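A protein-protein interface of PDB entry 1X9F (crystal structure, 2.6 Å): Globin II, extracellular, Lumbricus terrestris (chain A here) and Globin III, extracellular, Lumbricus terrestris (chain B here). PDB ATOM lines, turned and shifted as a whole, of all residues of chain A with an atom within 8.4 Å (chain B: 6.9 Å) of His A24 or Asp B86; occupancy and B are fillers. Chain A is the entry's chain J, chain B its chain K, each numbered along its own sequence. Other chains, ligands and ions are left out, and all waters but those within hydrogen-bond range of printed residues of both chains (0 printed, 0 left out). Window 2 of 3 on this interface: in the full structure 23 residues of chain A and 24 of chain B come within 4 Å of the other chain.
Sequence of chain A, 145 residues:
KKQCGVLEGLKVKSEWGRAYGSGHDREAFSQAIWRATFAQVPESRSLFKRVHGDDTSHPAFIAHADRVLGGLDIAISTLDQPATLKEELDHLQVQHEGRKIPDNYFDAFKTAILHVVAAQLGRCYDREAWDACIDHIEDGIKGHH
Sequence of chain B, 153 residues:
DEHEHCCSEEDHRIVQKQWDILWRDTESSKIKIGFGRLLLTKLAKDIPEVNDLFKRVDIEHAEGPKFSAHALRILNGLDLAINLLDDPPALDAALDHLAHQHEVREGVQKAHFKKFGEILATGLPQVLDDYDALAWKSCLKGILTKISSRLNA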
ATOM      1  N   TYR A  20     -11.223   7.718 -25.027  1.00  0.00           N
ATOM      2  CA  TYR A  20     -10.448   7.297 -23.861  1.00  0.00           C
ATOM      3  C   TYR A  20      -9.713   8.436 -23.138  1.00  0.00           C
ATOM      4  O   TYR A  20      -9.745   8.502 -21.907  1.00  0.00           O
ATOM      5  CB  TYR A  20      -9.477   6.192 -24.275  1.00  0.00           C
ATOM      6  CG  TYR A  20      -8.783   5.449 -23.158  1.00  0.00           C
ATOM      7  CD1 TYR A  20      -7.525   4.894 -23.371  1.00  0.00           C
ATOM      8  CD2 TYR A  20      -9.376   5.276 -21.907  1.00  0.00           C
ATOM      9  CE1 TYR A  20      -6.868   4.195 -22.375  1.00  0.00           C
ATOM     10  CE2 TYR A  20      -8.724   4.576 -20.899  1.00  0.00           C
ATOM     11  CZ  TYR A  20      -7.471   4.041 -21.140  1.00  0.00           C
ATOM     12  OH  TYR A  20      -6.812   3.346 -20.151  1.00  0.00           O
ATOM     13  N   GLY A  21      -9.056   9.319 -23.890  1.00  0.00           N
ATOM     14  CA  GLY A  21      -8.380  10.487 -23.301  1.00  0.00           C
ATOM     15  C   GLY A  21      -7.297  10.133 -22.297  1.00  0.00           C
ATOM     16  O   GLY A  21      -6.741   9.030 -22.341  1.00  0.00           O
ATOM     17  N   SER A  22      -6.996  11.062 -21.389  1.00  0.00           N
ATOM     18  CA  SER A  22      -5.908  10.875 -20.423  1.00  0.00           C
ATOM     19  C   SER A  22      -6.056  11.759 -19.190  1.00  0.00           C
ATOM     20  O   SER A  22      -6.900  12.662 -19.167  1.00  0.00           O
ATOM     21  CB  SER A  22      -4.550  11.122 -21.091  1.00  0.00           C
ATOM     22  OG  SER A  22      -4.420  12.468 -21.510  1.00  0.00           O
ATOM     23  N   GLY A  23      -5.242  11.492 -18.170  1.00  0.00           N
ATOM     24  CA  GLY A  23      -5.303  12.232 -16.910  1.00  0.00           C
ATOM     25  C   GLY A  23      -6.712  12.318 -16.347  1.00  0.00           C
ATOM     26  O   GLY A  23      -7.425  11.312 -16.278  1.00  0.00           O
ATOM     27  N   HIS A  24      -7.111  13.528 -15.964  1.00  0.00           N
ATOM     28  CA  HIS A  24      -8.410  13.765 -15.340  1.00  0.00           C
ATOM     29  C   HIS A  24      -9.592  13.323 -16.214  1.00  0.00           C
ATOM     30  O   HIS A  24     -10.552  12.740 -15.701  1.00  0.00           O
ATOM     31  CB  HIS A  24      -8.543  15.233 -14.907  1.00  0.00           C
ATOM     32  CG  HIS A  24      -7.707  15.589 -13.709  1.00  0.00           C
ATOM     33  ND1 HIS A  24      -7.691  14.826 -12.560  1.00  0.00           N
ATOM     34  CD2 HIS A  24      -6.876  16.633 -13.475  1.00  0.00           C
ATOM     35  CE1 HIS A  24      -6.877  15.375 -11.676  1.00  0.00           C
ATOM     36  NE2 HIS A  24      -6.371  16.475 -12.205  1.00  0.00           N
ATOM     37  N   ASP A  25      -9.508  13.585 -17.521  1.00  0.00           N
ATOM     38  CA  ASP A  25     -10.523  13.122 -18.482  1.00  0.00           C
ATOM     39  C   ASP A  25     -10.703  11.615 -18.431  1.00  0.00           C
ATOM     40  O   ASP A  25     -11.821  11.125 -18.570  1.00  0.00           O
ATOM     41  CB  ASP A  25     -10.159  13.515 -19.916  1.00  0.00           C
ATOM     42  CG  ASP A  25      -9.964  15.001 -20.080  1.00  0.00           C
ATOM     43  OD1 ASP A  25     -10.885  15.770 -19.719  1.00  0.00           O
ATOM     44  OD2 ASP A  25      -8.924  15.501 -20.566  1.00  0.00           O
ATOM     45  N   ARG A  26      -9.600  10.886 -18.248  1.00  0.00           N
ATOM     46  CA  ARG A  26      -9.646   9.426 -18.204  1.00  0.00           C
ATOM     47  C   ARG A  26     -10.272   8.944 -16.906  1.00  0.00           C
ATOM     48  O   ARG A  26     -11.068   8.009 -16.915  1.00  0.00           O
ATOM     49  CB  ARG A  26      -8.252   8.812 -18.392  1.00  0.00           C
ATOM     50  CG  ARG A  26      -8.260   7.290 -18.541  1.00  0.00           C
ATOM     51  CD  ARG A  26      -6.891   6.670 -18.746  1.00  0.00           C
ATOM     52  NE  ARG A  26      -6.314   7.029 -20.040  1.00  0.00           N
ATOM     53  CZ  ARG A  26      -5.123   6.630 -20.472  1.00  0.00           C
ATOM     54  NH1 ARG A  26      -4.365   5.840 -19.719  1.00  0.00           N
ATOM     55  NH2 ARG A  26      -4.687   7.014 -21.664  1.00  0.00           N
ATOM     56  N   GLU A  27      -9.914   9.579 -15.795  1.00  0.00           N
ATOM     57  CA  GLU A  27     -10.536   9.273 -14.518  1.00  0.00           C
ATOM     58  C   GLU A  27     -12.047   9.449 -14.593  1.00  0.00           C
ATOM     59  O   GLU A  27     -12.802   8.576 -14.157  1.00  0.00           O
ATOM     60  CB  GLU A  27      -9.969  10.173 -13.431  1.00  0.00           C
ATOM     61  CG  GLU A  27      -8.678   9.641 -12.843  1.00  0.00           C
ATOM     62  CD  GLU A  27      -8.200  10.462 -11.667  1.00  0.00           C
ATOM     63  OE1 GLU A  27      -7.974  11.679 -11.837  1.00  0.00           O
ATOM     64  OE2 GLU A  27      -8.037   9.889 -10.573  1.00  0.00           O
ATOM     65  N   ALA A  28     -12.471  10.579 -15.160  1.00  0.00           N
ATOM     66  CA  ALA A  28     -13.888  10.917 -15.281  1.00  0.00           C
ATOM     67  C   ALA A  28     -14.599   9.914 -16.173  1.00  0.00           C
ATOM     68  O   ALA A  28     -15.695   9.455 -15.845  1.00  0.00           O
ATOM     69  CB  ALA A  28     -14.052  12.331 -15.833  1.00  0.00           C
ATOM     70  N   PHE A  29     -13.963   9.587 -17.296  1.00  0.00           N
ATOM     71  CA  PHE A  29     -14.457   8.597 -18.254  1.00  0.00           C
ATOM     72  C   PHE A  29     -14.633   7.237 -17.580  1.00  0.00           C
ATOM     73  O   PHE A  29     -15.684   6.599 -17.706  1.00  0.00           O
ATOM     74  CB  PHE A  29     -13.457   8.500 -19.411  1.00  0.00           C
ATOM     75  CG  PHE A  29     -13.897   7.619 -20.544  1.00  0.00           C
ATOM     76  CD1 PHE A  29     -14.970   7.975 -21.356  1.00  0.00           C
ATOM     77  CD2 PHE A  29     -13.201   6.453 -20.834  1.00  0.00           C
ATOM     78  CE1 PHE A  29     -15.363   7.157 -22.426  1.00  0.00           C
ATOM     79  CE2 PHE A  29     -13.581   5.630 -21.899  1.00  0.00           C
ATOM     80  CZ  PHE A  29     -14.665   5.982 -22.697  1.00  0.00           C
ATOM     81  N   SER A  30     -13.590   6.817 -16.863  1.00  0.00           N
ATOM     82  CA  SER A  30     -13.601   5.597 -16.063  1.00  0.00           C
ATOM     83  C   SER A  30     -14.778   5.578 -15.104  1.00  0.00           C
ATOM     84  O   SER A  30     -15.443   4.550 -14.948  1.00  0.00           O
ATOM     85  CB  SER A  30     -12.299   5.462 -15.261  1.00  0.00           C
ATOM     86  OG  SER A  30     -11.212   5.072 -16.095  1.00  0.00           O
ATOM     87  N   GLN A  31     -15.029   6.714 -14.463  1.00  0.00           N
ATOM     88  CA  GLN A  31     -16.091   6.800 -13.471  1.00  0.00           C
ATOM     89  C   GLN A  31     -17.447   6.775 -14.135  1.00  0.00           C
ATOM     90  O   GLN A  31     -18.335   6.038 -13.703  1.00  0.00           O
ATOM     91  CB  GLN A  31     -15.952   8.067 -12.635  1.00  0.00           C
ATOM     92  CG  GLN A  31     -14.774   8.039 -11.695  1.00  0.00           C
ATOM     93  CD  GLN A  31     -14.657   9.307 -10.888  1.00  0.00           C
ATOM     94  OE1 GLN A  31     -15.136   9.365  -9.754  1.00  0.00           O
ATOM     95  NE2 GLN A  31     -14.032  10.331 -11.466  1.00  0.00           N
ATOM     96  N   ILE A  62     -11.260   4.437  -8.162  1.00  0.00           N
ATOM     97  CA  ILE A  62     -10.726   5.060  -9.371  1.00  0.00           C
ATOM     98  C   ILE A  62      -9.678   4.128  -9.954  1.00  0.00           C
ATOM     99  O   ILE A  62      -9.717   3.797 -11.141  1.00  0.00           O
ATOM    100  CB  ILE A  62     -10.098   6.437  -9.080  1.00  0.00           C
ATOM    101  CG1 ILE A  62     -11.123   7.397  -8.465  1.00  0.00           C
ATOM    102  CG2 ILE A  62      -9.477   7.021 -10.351  1.00  0.00           C
ATOM    103  CD1 ILE A  62     -12.313   7.689  -9.342  1.00  0.00           C
ATOM    104  N   ASP A  66      -9.897   2.640 -13.630  1.00  0.00           N
ATOM    105  CA  ASP A  66      -8.815   2.855 -14.596  1.00  0.00           C
ATOM    106  C   ASP A  66      -8.189   1.510 -14.995  1.00  0.00           C
ATOM    107  O   ASP A  66      -7.823   1.309 -16.153  1.00  0.00           O
ATOM    108  CB  ASP A  66      -7.742   3.805 -14.033  1.00  0.00           C
ATOM    109  CG  ASP A  66      -7.945   5.266 -14.457  1.00  0.00           C
ATOM    110  OD1 ASP A  66      -6.937   6.007 -14.578  1.00  0.00           O
ATOM    111  OD2 ASP A  66      -9.064   5.765 -14.689  1.00  0.00           O
ATOM    112  N   GLU B   9       4.605  19.010  -8.882  1.00  0.00           N
ATOM    113  CA  GLU B   9       3.484  19.276  -9.778  1.00  0.00           C
ATOM    114  C   GLU B   9       3.969  19.381 -11.214  1.00  0.00           C
ATOM    115  O   GLU B   9       3.510  18.631 -12.076  1.00  0.00           O
ATOM    116  CB  GLU B   9       2.747  20.565  -9.392  1.00  0.00           C
ATOM    117  CG  GLU B   9       1.967  20.486  -8.086  1.00  0.00           C
ATOM    118  CD  GLU B   9       0.874  19.427  -8.091  1.00  0.00           C
ATOM    119  OE1 GLU B   9       0.622  18.842  -7.015  1.00  0.00           O
ATOM    120  OE2 GLU B   9       0.265  19.176  -9.156  1.00  0.00           O
ATOM    121  N   HIS B  12       5.580  16.010 -12.822  1.00  0.00           N
ATOM    122  CA  HIS B  12       4.684  14.990 -13.340  1.00  0.00           C
ATOM    123  C   HIS B  12       3.886  15.497 -14.536  1.00  0.00           C
ATOM    124  O   HIS B  12       3.474  14.707 -15.385  1.00  0.00           O
ATOM    125  CB  HIS B  12       3.786  14.399 -12.238  1.00  0.00           C
ATOM    126  CG  HIS B  12       2.594  15.238 -11.886  1.00  0.00           C
ATOM    127  ND1 HIS B  12       2.313  15.625 -10.592  1.00  0.00           N
ATOM    128  CD2 HIS B  12       1.590  15.733 -12.650  1.00  0.00           C
ATOM    129  CE1 HIS B  12       1.199  16.338 -10.578  1.00  0.00           C
ATOM    130  NE2 HIS B  12       0.743  16.421 -11.816  1.00  0.00           N
ATOM    131  N   GLN B  16       3.783  13.551 -18.024  1.00  0.00           N
ATOM    132  CA  GLN B  16       2.545  13.229 -18.729  1.00  0.00           C
ATOM    133  C   GLN B  16       2.525  13.753 -20.161  1.00  0.00           C
ATOM    134  O   GLN B  16       2.101  13.042 -21.073  1.00  0.00           O
ATOM    135  CB  GLN B  16       1.333  13.747 -17.965  1.00  0.00           C
ATOM    136  CG  GLN B  16       1.120  13.033 -16.651  1.00  0.00           C
ATOM    137  CD  GLN B  16      -0.065  13.580 -15.903  1.00  0.00           C
ATOM    138  OE1 GLN B  16      -0.326  14.786 -15.929  1.00  0.00           O
ATOM    139  NE2 GLN B  16      -0.799  12.698 -15.228  1.00  0.00           N
ATOM    140  N   ALA B  81      -0.137   4.374 -14.091  1.00  0.00           N
ATOM    141  CA  ALA B  81       0.566   5.165 -13.083  1.00  0.00           C
ATOM    142  C   ALA B  81       0.828   6.578 -13.577  1.00  0.00           C
ATOM    143  O   ALA B  81       0.511   7.544 -12.874  1.00  0.00           O
ATOM    144  CB  ALA B  81       1.870   4.489 -12.670  1.00  0.00           C
ATOM    145  N   ILE B  82       1.386   6.703 -14.785  1.00  0.00           N
ATOM    146  CA  ILE B  82       1.610   8.030 -15.373  1.00  0.00           C
ATOM    147  C   ILE B  82       0.319   8.847 -15.451  1.00  0.00           C
ATOM    148  O   ILE B  82       0.307  10.023 -15.076  1.00  0.00           O
ATOM    149  CB  ILE B  82       2.321   7.962 -16.746  1.00  0.00           C
ATOM    150  CG1 ILE B  82       3.745   7.430 -16.568  1.00  0.00           C
ATOM    151  CG2 ILE B  82       2.353   9.347 -17.413  1.00  0.00           C
ATOM    152  CD1 ILE B  82       4.510   7.211 -17.856  1.00  0.00           C
ATOM    153  N   ASN B  83      -0.762   8.229 -15.913  1.00  0.00           N
ATOM    154  CA  ASN B  83      -2.023   8.953 -16.034  1.00  0.00           C
ATOM    155  C   ASN B  83      -2.704   9.251 -14.713  1.00  0.00           C
ATOM    156  O   ASN B  83      -3.723   9.939 -14.684  1.00  0.00           O
ATOM    157  CB  ASN B  83      -2.988   8.232 -16.962  1.00  0.00           C
ATOM    158  CG  ASN B  83      -2.742   8.565 -18.403  1.00  0.00           C
ATOM    159  OD1 ASN B  83      -3.397   9.439 -18.965  1.00  0.00           O
ATOM    160  ND2 ASN B  83      -1.777   7.885 -19.013  1.00  0.00           N
ATOM    161  N   LEU B  84      -2.154   8.736 -13.620  1.00  0.00           N
ATOM    162  CA  LEU B  84      -2.699   9.051 -12.310  1.00  0.00           C
ATOM    163  C   LEU B  84      -1.760   9.907 -11.473  1.00  0.00           C
ATOM    164  O   LEU B  84      -2.029  10.146 -10.294  1.00  0.00           O
ATOM    165  CB  LEU B  84      -3.084   7.772 -11.556  1.00  0.00           C
ATOM    166  CG  LEU B  84      -4.361   7.057 -12.012  1.00  0.00           C
ATOM    167  CD1 LEU B  84      -4.551   5.742 -11.261  1.00  0.00           C
ATOM    168  CD2 LEU B  84      -5.589   7.937 -11.822  1.00  0.00           C
ATOM    169  N   LEU B  85      -0.669  10.379 -12.074  1.00  0.00           N
ATOM    170  CA  LEU B  85       0.317  11.176 -11.336  1.00  0.00           C
ATOM    171  C   LEU B  85      -0.297  12.438 -10.744  1.00  0.00           C
ATOM    172  O   LEU B  85       0.126  12.903  -9.684  1.00  0.00           O
ATOM    173  CB  LEU B  85       1.496  11.533 -12.236  1.00  0.00           C
ATOM    174  CG  LEU B  85       2.502  10.403 -12.451  1.00  0.00           C
ATOM    175  CD1 LEU B  85       3.488  10.760 -13.558  1.00  0.00           C
ATOM    176  CD2 LEU B  85       3.238  10.080 -11.153  1.00  0.00           C
ATOM    177  N   ASP B  86      -1.307  12.970 -11.428  1.00  0.00           N
ATOM    178  CA  ASP B  86      -2.010  14.169 -10.982  1.00  0.00           C
ATOM    179  C   ASP B  86      -3.088  13.876  -9.934  1.00  0.00           C
ATOM    180  O   ASP B  86      -3.889  14.757  -9.590  1.00  0.00           O
ATOM    181  CB  ASP B  86      -2.623  14.914 -12.178  1.00  0.00           C
ATOM    182  CG  ASP B  86      -2.882  16.385 -11.874  1.00  0.00           C
ATOM    183  OD1 ASP B  86      -3.698  17.008 -12.591  1.00  0.00           O
ATOM    184  OD2 ASP B  86      -2.321  17.006 -10.939  1.00  0.00           O
ATOM    185  N   ASP B  87      -3.106  12.646  -9.425  1.00  0.00           N
ATOM    186  CA  ASP B  87      -4.062  12.237  -8.397  1.00  0.00           C
ATOM    187  C   ASP B  87      -3.398  11.277  -7.407  1.00  0.00           C
ATOM    188  O   ASP B  87      -3.657  10.068  -7.434  1.00  0.00           O
ATOM    189  CB  ASP B  87      -5.281  11.581  -9.043  1.00  0.00           C
ATOM    190  CG  ASP B  87      -6.432  11.375  -8.068  1.00  0.00           C
ATOM    191  OD1 ASP B  87      -6.199  11.115  -6.867  1.00  0.00           O
ATOM    192  OD2 ASP B  87      -7.626  11.451  -8.424  1.00  0.00           O
ATOM    193  N   PRO B  88      -2.543  11.812  -6.535  1.00  0.00           N
ATOM    194  CA  PRO B  88      -1.708  10.979  -5.659  1.00  0.00           C
ATOM    195  C   PRO B  88      -2.395   9.801  -4.923  1.00  0.00           C
ATOM    196  O   PRO B  88      -1.852   8.691  -4.959  1.00  0.00           O
ATOM    197  CB  PRO B  88      -1.086  11.984  -4.668  1.00  0.00           C
ATOM    198  CG  PRO B  88      -1.691  13.320  -4.982  1.00  0.00           C
ATOM    199  CD  PRO B  88      -2.283  13.253  -6.345  1.00  0.00           C
ATOM    200  N   PRO B  89      -3.548  10.011  -4.273  1.00  0.00           N
ATOM    201  CA  PRO B  89      -4.190   8.925  -3.528  1.00  0.00           C
ATOM    202  C   PRO B  89      -4.676   7.792  -4.438  1.00  0.00           C
ATOM    203  O   PRO B  89      -4.508   6.615  -4.094  1.00  0.00           O
ATOM    204  CB  PRO B  89      -5.361   9.617  -2.809  1.00  0.00           C
ATOM    205  CG  PRO B  89      -5.637  10.843  -3.598  1.00  0.00           C
ATOM    206  CD  PRO B  89      -4.327  11.262  -4.182  1.00  0.00           C
ATOM    207  N   LEU B  91      -3.301   7.164  -7.288  1.00  0.00           N
ATOM    208  CA  LEU B  91      -2.045   6.593  -7.760  1.00  0.00           C
ATOM    209  C   LEU B  91      -1.539   5.555  -6.776  1.00  0.00           C
ATOM    210  O   LEU B  91      -1.168   4.446  -7.167  1.00  0.00           O
ATOM    211  CB  LEU B  91      -0.981   7.679  -7.974  1.00  0.00           C
ATOM    212  CG  LEU B  91       0.424   7.183  -8.340  1.00  0.00           C
ATOM    213  CD1 LEU B  91       0.386   6.434  -9.681  1.00  0.00           C
ATOM    214  CD2 LEU B  91       1.423   8.337  -8.396  1.00  0.00           C
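The backbone carbonyl oxygen (O) of Gly A21 lies within hydrogen-bond range of the guanidinium group (NH2) of Arg A26, 3.0 Å away. A ring nitrogen (ND1) of His A24 lies within hydrogen-bond range of the side-chain carboxylate of Glu A27 (3.2 Å). O of Arg A26 sits at hydrogen-bond distance from OG of Ser A30 (3.1 Å). The backbone carbonyl oxygen (O) of Glu A27 sits close to the side-chain amide nitrogen (NE2) of Gln A31. OD2 of Asp A66 sits at hydrogen-bond distance from OG of Ser A30, at 2.7 Å. The side-chain carboxylate of Asp B86 is in hydrogen-bond range of a ring nitrogen (NE2) of His B12 (3.2 Å).
Among the printed residues, merely in contact across the chains: Ser A22 with Asn B83 (2.9 Å), Glu A27 with Leu B84 (3.4 Å) and Asp A66 with Leu B84 (3.6 Å).
Printed residues of chain A that touch a printed residue of chain B: Ser A22, Gly A23, His A24, Arg A26, Glu A27 and Asp A66. Of the 13 printed residues of chain B, 4 touch a printed residue of chain A. Hydrophobic or aromatic side chains of chain B that line the printed part of chain A: Leu B84. Among the printed residues, 7 pairs touch across the chains.
The backbone NH (N) of Gly A23 lies within hydrogen-bond range of the side-chain amide oxygen (OD1) of Asn B83 (2.9 Å). The side-chain carboxylate (OD1) of Asp B86 sits at hydrogen-bond distance from a ring nitrogen (NE2) of His A24, at 2.8 Å. ND2 of Asn B83 lies close to NH1 of Arg A26 (3.4 Å). The side-chain carboxylate (OE2) of Glu A27 sits close to the side-chain carboxylate (OD2) of Asp B87 (2.7 Å).
Of the printed residues of chain B, Ser A22 touches Asn B83. Of the printed residues of chain B, Gly A23 touches Asn B83. Of chain B, only Asp B86 comes within 4 Å of His A24. Of the printed residues of chain B, Asp A66 touches Leu B84. Ile B82 touches none of the printed residues of chain A. Of the printed residues of chain A, Asn B83 touches Ser A22, Gly A23 and Arg A26. Of the printed residues of chain A, Asp B86 touches His A24. Printed residues of chain A within 4 Å of Asp B87: Glu A27. The nearest residue of chain B that does not touch His A24 is Asp B87 (4.9 Å). The nearest residue of chain A that does not touch Asp B86 is Glu A27 (5.6 Å).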
